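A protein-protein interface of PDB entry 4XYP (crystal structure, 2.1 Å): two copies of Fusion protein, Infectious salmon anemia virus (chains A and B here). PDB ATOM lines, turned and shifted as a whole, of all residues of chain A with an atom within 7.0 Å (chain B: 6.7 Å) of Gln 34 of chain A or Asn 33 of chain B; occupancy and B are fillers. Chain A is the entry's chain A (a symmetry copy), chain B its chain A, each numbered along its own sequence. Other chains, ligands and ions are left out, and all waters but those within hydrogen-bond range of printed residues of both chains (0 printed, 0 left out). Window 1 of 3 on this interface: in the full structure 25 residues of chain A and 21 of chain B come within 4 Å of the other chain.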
ATOM      1  N   ILE A  29      -4.568   3.695  -5.995  1.00  0.00           N
ATOM      2  CA  ILE A  29      -3.210   4.143  -6.256  1.00  0.00           C
ATOM      3  C   ILE A  29      -2.826   5.232  -5.267  1.00  0.00           C
ATOM      4  O   ILE A  29      -1.706   5.242  -4.756  1.00  0.00           O
ATOM      5  CB  ILE A  29      -3.038   4.690  -7.711  1.00  0.00           C
ATOM      6  CG1 ILE A  29      -3.348   3.591  -8.740  1.00  0.00           C
ATOM      7  CG2 ILE A  29      -1.620   5.215  -7.935  1.00  0.00           C
ATOM      8  CD1 ILE A  29      -3.417   4.091 -10.199  1.00  0.00           C
ATOM      9  N   ALA A  30      -3.742   6.168  -5.041  1.00  0.00           N
ATOM     10  CA  ALA A  30      -3.448   7.328  -4.203  1.00  0.00           C
ATOM     11  C   ALA A  30      -3.232   6.889  -2.759  1.00  0.00           C
ATOM     12  O   ALA A  30      -2.355   7.411  -2.066  1.00  0.00           O
ATOM     13  CB  ALA A  30      -4.542   8.339  -4.297  1.00  0.00           C
ATOM     14  N   TYR A  31      -3.974   5.875  -2.323  1.00  0.00           N
ATOM     15  CA  TYR A  31      -3.767   5.342  -0.977  1.00  0.00           C
ATOM     16  C   TYR A  31      -2.447   4.598  -0.864  1.00  0.00           C
ATOM     17  O   TYR A  31      -1.789   4.693   0.167  1.00  0.00           O
ATOM     18  CB  TYR A  31      -4.921   4.444  -0.548  1.00  0.00           C
ATOM     19  CG  TYR A  31      -6.043   5.270   0.054  1.00  0.00           C
ATOM     20  CD1 TYR A  31      -5.802   6.110   1.142  1.00  0.00           C
ATOM     21  CD2 TYR A  31      -7.328   5.221  -0.457  1.00  0.00           C
ATOM     22  CE1 TYR A  31      -6.811   6.871   1.696  1.00  0.00           C
ATOM     23  CE2 TYR A  31      -8.349   5.980   0.095  1.00  0.00           C
ATOM     24  CZ  TYR A  31      -8.080   6.803   1.166  1.00  0.00           C
ATOM     25  OH  TYR A  31      -9.093   7.552   1.713  1.00  0.00           O
ATOM     26  N   MET A  32      -2.057   3.889  -1.919  1.00  0.00           N
ATOM     27  CA  MET A  32      -0.749   3.271  -1.986  1.00  0.00           C
ATOM     28  C   MET A  32       0.371   4.317  -1.948  1.00  0.00           C
ATOM     29  O   MET A  32       1.338   4.159  -1.239  1.00  0.00           O
ATOM     30  CB  MET A  32      -0.615   2.438  -3.257  1.00  0.00           C
ATOM     31  CG  MET A  32      -1.133   0.982  -3.144  1.00  0.00           C
ATOM     32  SD  MET A  32      -1.254   0.159  -4.753  1.00  0.00           S
ATOM     33  CE  MET A  32       0.422   0.270  -5.344  1.00  0.00           C
ATOM     34  N   ASN A  33       0.231   5.381  -2.719  1.00  0.00           N
ATOM     35  CA  ASN A  33       1.213   6.439  -2.738  1.00  0.00           C
ATOM     36  C   ASN A  33       1.353   7.119  -1.381  1.00  0.00           C
ATOM     37  O   ASN A  33       2.460   7.461  -0.955  1.00  0.00           O
ATOM     38  CB  ASN A  33       0.844   7.465  -3.834  1.00  0.00           C
ATOM     39  CG  ASN A  33       1.086   6.922  -5.226  1.00  0.00           C
ATOM     40  OD1 ASN A  33       1.758   5.911  -5.383  1.00  0.00           O
ATOM     41  ND2 ASN A  33       0.537   7.577  -6.241  1.00  0.00           N
ATOM     42  N   GLN A  34       0.244   7.272  -0.672  1.00  0.00           N
ATOM     43  CA  GLN A  34       0.278   7.923   0.630  1.00  0.00           C
ATOM     44  C   GLN A  34       1.112   7.076   1.583  1.00  0.00           C
ATOM     45  O   GLN A  34       1.979   7.592   2.294  1.00  0.00           O
ATOM     46  CB  GLN A  34      -1.128   8.123   1.165  1.00  0.00           C
ATOM     47  CG  GLN A  34      -1.247   9.147   2.220  1.00  0.00           C
ATOM     48  CD  GLN A  34      -2.677   9.275   2.646  1.00  0.00           C
ATOM     49  OE1 GLN A  34      -3.394   8.275   2.755  1.00  0.00           O
ATOM     50  NE2 GLN A  34      -3.119  10.501   2.849  1.00  0.00           N
ATOM     51  N   ALA A  35       0.900   5.765   1.550  1.00  0.00           N
ATOM     52  CA  ALA A  35       1.652   4.864   2.422  1.00  0.00           C
ATOM     53  C   ALA A  35       3.145   4.827   2.057  1.00  0.00           C
ATOM     54  O   ALA A  35       4.016   4.763   2.939  1.00  0.00           O
ATOM     55  CB  ALA A  35       1.066   3.454   2.362  1.00  0.00           C
ATOM     56  N   SER A  36       3.460   4.842   0.760  1.00  0.00           N
ATOM     57  CA  SER A  36       4.864   4.860   0.324  1.00  0.00           C
ATOM     58  C   SER A  36       5.580   6.146   0.692  1.00  0.00           C
ATOM     59  O   SER A  36       6.765   6.142   1.101  1.00  0.00           O
ATOM     60  CB  SER A  36       4.977   4.674  -1.184  1.00  0.00           C
ATOM     61  OG  SER A  36       4.545   3.383  -1.544  1.00  0.00           O
ATOM     62  N   SER A  37       4.890   7.264   0.528  1.00  0.00           N
ATOM     63  CA  SER A  37       5.524   8.537   0.864  1.00  0.00           C
ATOM     64  C   SER A  37       5.691   8.657   2.389  1.00  0.00           C
ATOM     65  O   SER A  37       6.678   9.216   2.853  1.00  0.00           O
ATOM     66  CB  SER A  37       4.732   9.711   0.267  1.00  0.00           C
ATOM     67  OG  SER A  37       3.487   9.846   0.925  1.00  0.00           O
ATOM     68  N   LEU A  38       4.778   8.127   3.194  1.00  0.00           N
ATOM     69  CA  LEU A  38       5.033   8.091   4.638  1.00  0.00           C
ATOM     70  C   LEU A  38       6.256   7.221   4.971  1.00  0.00           C
ATOM     71  O   LEU A  38       7.143   7.631   5.723  1.00  0.00           O
ATOM     72  CB  LEU A  38       3.807   7.572   5.383  1.00  0.00           C
ATOM     73  CG  LEU A  38       4.063   7.277   6.857  1.00  0.00           C
ATOM     74  CD1 LEU A  38       4.387   8.575   7.559  1.00  0.00           C
ATOM     75  CD2 LEU A  38       2.889   6.572   7.492  1.00  0.00           C
ATOM     76  N   GLN A  39       6.292   6.004   4.438  1.00  0.00           N
ATOM     77  CA  GLN A  39       7.446   5.142   4.610  1.00  0.00           C
ATOM     78  C   GLN A  39       8.760   5.787   4.232  1.00  0.00           C
ATOM     79  O   GLN A  39       9.753   5.662   4.966  1.00  0.00           O
ATOM     80  CB  GLN A  39       7.325   3.872   3.785  1.00  0.00           C
ATOM     81  CG  GLN A  39       8.402   2.899   4.099  1.00  0.00           C
ATOM     82  CD  GLN A  39       8.222   1.616   3.350  1.00  0.00           C
ATOM     83  OE1 GLN A  39       7.420   0.773   3.745  1.00  0.00           O
ATOM     84  NE2 GLN A  39       8.961   1.459   2.260  1.00  0.00           N
ATOM     85  N   ASN A  40       8.800   6.399   3.051  1.00  0.00           N
ATOM     86  CA  ASN A  40      10.007   7.112   2.623  1.00  0.00           C
ATOM     87  C   ASN A  40      10.383   8.247   3.564  1.00  0.00           C
ATOM     88  O   ASN A  40      11.570   8.431   3.896  1.00  0.00           O
ATOM     89  CB  ASN A  40       9.842   7.640   1.191  1.00  0.00           C
ATOM     90  CG  ASN A  40       9.767   6.509   0.162  1.00  0.00           C
ATOM     91  OD1 ASN A  40      10.188   5.406   0.443  1.00  0.00           O
ATOM     92  ND2 ASN A  40       9.231   6.792  -1.018  1.00  0.00           N
ATOM     93  N   ARG B  28      -7.503  15.679  -3.358  1.00  0.00           N
ATOM     94  CA  ARG B  28      -6.862  16.251  -2.191  1.00  0.00           C
ATOM     95  C   ARG B  28      -5.679  15.366  -1.779  1.00  0.00           C
ATOM     96  O   ARG B  28      -4.599  15.852  -1.422  1.00  0.00           O
ATOM     97  CB  ARG B  28      -7.872  16.405  -1.040  1.00  0.00           C
ATOM     98  N   ILE B  29      -5.882  14.052  -1.843  1.00  0.00           N
ATOM     99  CA  ILE B  29      -4.844  13.108  -1.461  1.00  0.00           C
ATOM    100  C   ILE B  29      -3.684  13.190  -2.440  1.00  0.00           C
ATOM    101  O   ILE B  29      -2.522  13.156  -2.034  1.00  0.00           O
ATOM    102  CB  ILE B  29      -5.373  11.636  -1.415  1.00  0.00           C
ATOM    103  CG1 ILE B  29      -6.500  11.501  -0.379  1.00  0.00           C
ATOM    104  CG2 ILE B  29      -4.246  10.661  -1.077  1.00  0.00           C
ATOM    105  CD1 ILE B  29      -7.231  10.142  -0.414  1.00  0.00           C
ATOM    106  N   ALA B  30      -4.008  13.250  -3.728  1.00  0.00           N
ATOM    107  CA  ALA B  30      -2.983  13.213  -4.769  1.00  0.00           C
ATOM    108  C   ALA B  30      -2.128  14.473  -4.706  1.00  0.00           C
ATOM    109  O   ALA B  30      -0.910  14.418  -4.892  1.00  0.00           O
ATOM    110  CB  ALA B  30      -3.604  13.052  -6.116  1.00  0.00           C
ATOM    111  N   TYR B  31      -2.746  15.600  -4.367  1.00  0.00           N
ATOM    112  CA  TYR B  31      -1.980  16.835  -4.204  1.00  0.00           C
ATOM    113  C   TYR B  31      -1.098  16.790  -2.968  1.00  0.00           C
ATOM    114  O   TYR B  31       0.019  17.295  -3.007  1.00  0.00           O
ATOM    115  CB  TYR B  31      -2.891  18.057  -4.163  1.00  0.00           C
ATOM    116  CG  TYR B  31      -3.195  18.542  -5.569  1.00  0.00           C
ATOM    117  CD1 TYR B  31      -2.161  18.879  -6.442  1.00  0.00           C
ATOM    118  CD2 TYR B  31      -4.496  18.658  -6.025  1.00  0.00           C
ATOM    119  CE1 TYR B  31      -2.422  19.316  -7.725  1.00  0.00           C
ATOM    120  CE2 TYR B  31      -4.768  19.099  -7.311  1.00  0.00           C
ATOM    121  CZ  TYR B  31      -3.727  19.421  -8.153  1.00  0.00           C
ATOM    122  OH  TYR B  31      -3.998  19.860  -9.425  1.00  0.00           O
ATOM    123  N   MET B  32      -1.585  16.174  -1.896  1.00  0.00           N
ATOM    124  CA  MET B  32      -0.777  15.930  -0.718  1.00  0.00           C
ATOM    125  C   MET B  32       0.409  15.011  -1.030  1.00  0.00           C
ATOM    126  O   MET B  32       1.516  15.275  -0.616  1.00  0.00           O
ATOM    127  CB  MET B  32      -1.620  15.303   0.388  1.00  0.00           C
ATOM    128  CG  MET B  32      -2.370  16.314   1.293  1.00  0.00           C
ATOM    129  SD  MET B  32      -3.597  15.518   2.360  1.00  0.00           S
ATOM    130  CE  MET B  32      -2.592  14.362   3.270  1.00  0.00           C
ATOM    131  N   ASN B  33       0.167  13.935  -1.755  1.00  0.00           N
ATOM    132  CA  ASN B  33       1.219  13.020  -2.129  1.00  0.00           C
ATOM    133  C   ASN B  33       2.281  13.684  -2.998  1.00  0.00           C
ATOM    134  O   ASN B  33       3.477  13.424  -2.846  1.00  0.00           O
ATOM    135  CB  ASN B  33       0.605  11.794  -2.847  1.00  0.00           C
ATOM    136  CG  ASN B  33      -0.140  10.889  -1.890  1.00  0.00           C
ATOM    137  OD1 ASN B  33       0.011  11.014  -0.682  1.00  0.00           O
ATOM    138  ND2 ASN B  33      -0.953   9.981  -2.416  1.00  0.00           N
ATOM    139  N   GLN B  34       1.857  14.582  -3.875  1.00  0.00           N
ATOM    140  CA  GLN B  34       2.796  15.259  -4.757  1.00  0.00           C
ATOM    141  C   GLN B  34       3.742  16.105  -3.914  1.00  0.00           C
ATOM    142  O   GLN B  34       4.961  16.072  -4.106  1.00  0.00           O
ATOM    143  CB  GLN B  34       2.058  16.113  -5.772  1.00  0.00           C
ATOM    144  CG  GLN B  34       2.844  16.469  -6.967  1.00  0.00           C
ATOM    145  CD  GLN B  34       2.006  17.283  -7.905  1.00  0.00           C
ATOM    146  OE1 GLN B  34       1.228  18.139  -7.473  1.00  0.00           O
ATOM    147  NE2 GLN B  34       2.119  16.999  -9.188  1.00  0.00           N
ATOM    148  N   ALA B  35       3.190  16.813  -2.935  1.00  0.00           N
ATOM    149  CA  ALA B  35       4.012  17.655  -2.067  1.00  0.00           C
ATOM    150  C   ALA B  35       4.960  16.819  -1.190  1.00  0.00           C
ATOM    151  O   ALA B  35       6.115  17.207  -0.952  1.00  0.00           O
ATOM    152  CB  ALA B  35       3.126  18.533  -1.185  1.00  0.00           C
ATOM    153  N   SER B  36       4.482  15.682  -0.682  1.00  0.00           N
ATOM    154  CA  SER B  36       5.336  14.798   0.126  1.00  0.00           C
ATOM    155  C   SER B  36       6.461  14.171  -0.676  1.00  0.00           C
ATOM    156  O   SER B  36       7.612  14.041  -0.197  1.00  0.00           O
ATOM    157  CB  SER B  36       4.526  13.674   0.758  1.00  0.00           C
ATOM    158  OG  SER B  36       3.625  14.200   1.702  1.00  0.00           O
ATOM    159  N   SER B  37       6.146  13.750  -1.891  1.00  0.00           N
ATOM    160  CA  SER B  37       7.186  13.136  -2.713  1.00  0.00           C
ATOM    161  C   SER B  37       8.205  14.200  -3.158  1.00  0.00           C
ATOM    162  O   SER B  37       9.391  13.907  -3.255  1.00  0.00           O
ATOM    163  CB  SER B  37       6.564  12.389  -3.903  1.00  0.00           C
ATOM    164  OG  SER B  37       6.001  13.308  -4.819  1.00  0.00           O
ATOM    165  N   LEU B  38       7.797  15.439  -3.403  1.00  0.00           N
ATOM    166  CA  LEU B  38       8.794  16.484  -3.651  1.00  0.00           C
ATOM    167  C   LEU B  38       9.689  16.711  -2.423  1.00  0.00           C
ATOM    168  O   LEU B  38      10.917  16.754  -2.528  1.00  0.00           O
ATOM    169  CB  LEU B  38       8.112  17.791  -4.046  1.00  0.00           C
ATOM    170  CG  LEU B  38       9.056  18.988  -4.090  1.00  0.00           C
ATOM    171  CD1 LEU B  38      10.066  18.765  -5.191  1.00  0.00           C
ATOM    172  CD2 LEU B  38       8.299  20.282  -4.275  1.00  0.00           C
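N of Gln 34 of chain A lies close to ND2 of Asn 33 of chain B, at 3.4 Å. O of Ala 30 of chain A lies within hydrogen-bond range of ND2 of Asn 33 of chain B (2.9 Å).
The backbone carbonyl oxygen of Asn 33 of chain A lies within hydrogen-bond range of the side-chain hydroxyl of Ser 37 of chain A (3.2 Å). The side-chain hydroxyl of Ser 37 of chain B sits at hydrogen-bond distance from the backbone carbonyl oxygen of Asn 33 of chain B (3.2 Å). The side-chain hydroxyl (OG) of Ser 36 of chain B lies within hydrogen-bond range of the backbone carbonyl oxygen (O) of Met 32 of chain B (3.3 Å). The side-chain hydroxyl of Ser 37 of chain A lies within hydrogen-bond range of the backbone carbonyl oxygen of Gln 34 of chain A (3.0 Å).
Among the printed residues, pairs that only touch across the chains: Ala 30 of chain A with Ile 29 of chain B (3.9 Å), Tyr 31 of chain A with Ile 29 of chain B (3.8 Å), Asn 33 of chain A with Asn 33 of chain B (3.4 Å), Gln 34 of chain A with Met 32 of chain B (3.9 Å) and Ser 37 of chain A with Ser 36 of chain B (3.97 Å).
Printed residues of chain B within 4 Å of Ala 30 of chain A: Ile 29 (3.9 Å) and Asn 33 (2.9 Å). Of the printed residues of chain B, Ser 37 of chain A touches Ser 36 (3.97 Å). Of the printed residues of chain A, Ile 29 of chain B touches Ala 30 and Tyr 31. Of the printed residues of chain A, Asn 33 of chain B touches Ala 30 (2.9 Å), Asn 33 (3.4 Å) and Gln 34 (3.4 Å). The nearest residue of chain B that does not touch Gln 34 of chain A is Ile 29 of chain B (4.1 Å). The nearest printed residue of chain A that does not touch Asn 33 of chain B is Ser 37 of chain A (4.004 Å). The nearest printed residue of chain A that does not touch Ile 29 of chain B is Gln 34 of chain A (4.1 Å).
Of the 12 printed residues of chain A, 5 touch a printed residue of chain B. Hydrophobic or aromatic side chains of chain A within 4 Å of the printed part of chain B: Ala 30 and Tyr 31. Printed residues of chain B that touch a printed residue of chain A: Ile 29, Met 32, Asn 33 and Ser 36.
Ala 30 of chain A touches Ile 29 of chain B, but with the chains exchanged Ile 29 of chain A does not touch Ala 30 of chain B (7.9 Å). Asn 33 of chain A touches its own counterpart, Asn 33 of chain B. Gln 34 of chain A touches Met 32 of chain B, but with the chains exchanged Met 32 of chain A does not touch Gln 34 of chain B (10.5 Å). Ser 37 of chain A touches Ser 36 of chain B, but with the chains exchanged Ser 36 of chain A does not touch Ser 37 of chain B (7.8 Å). Of the 7 pairs that touch across the chains among the printed residues, 1 has its exchanged pair printed and touching as well.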
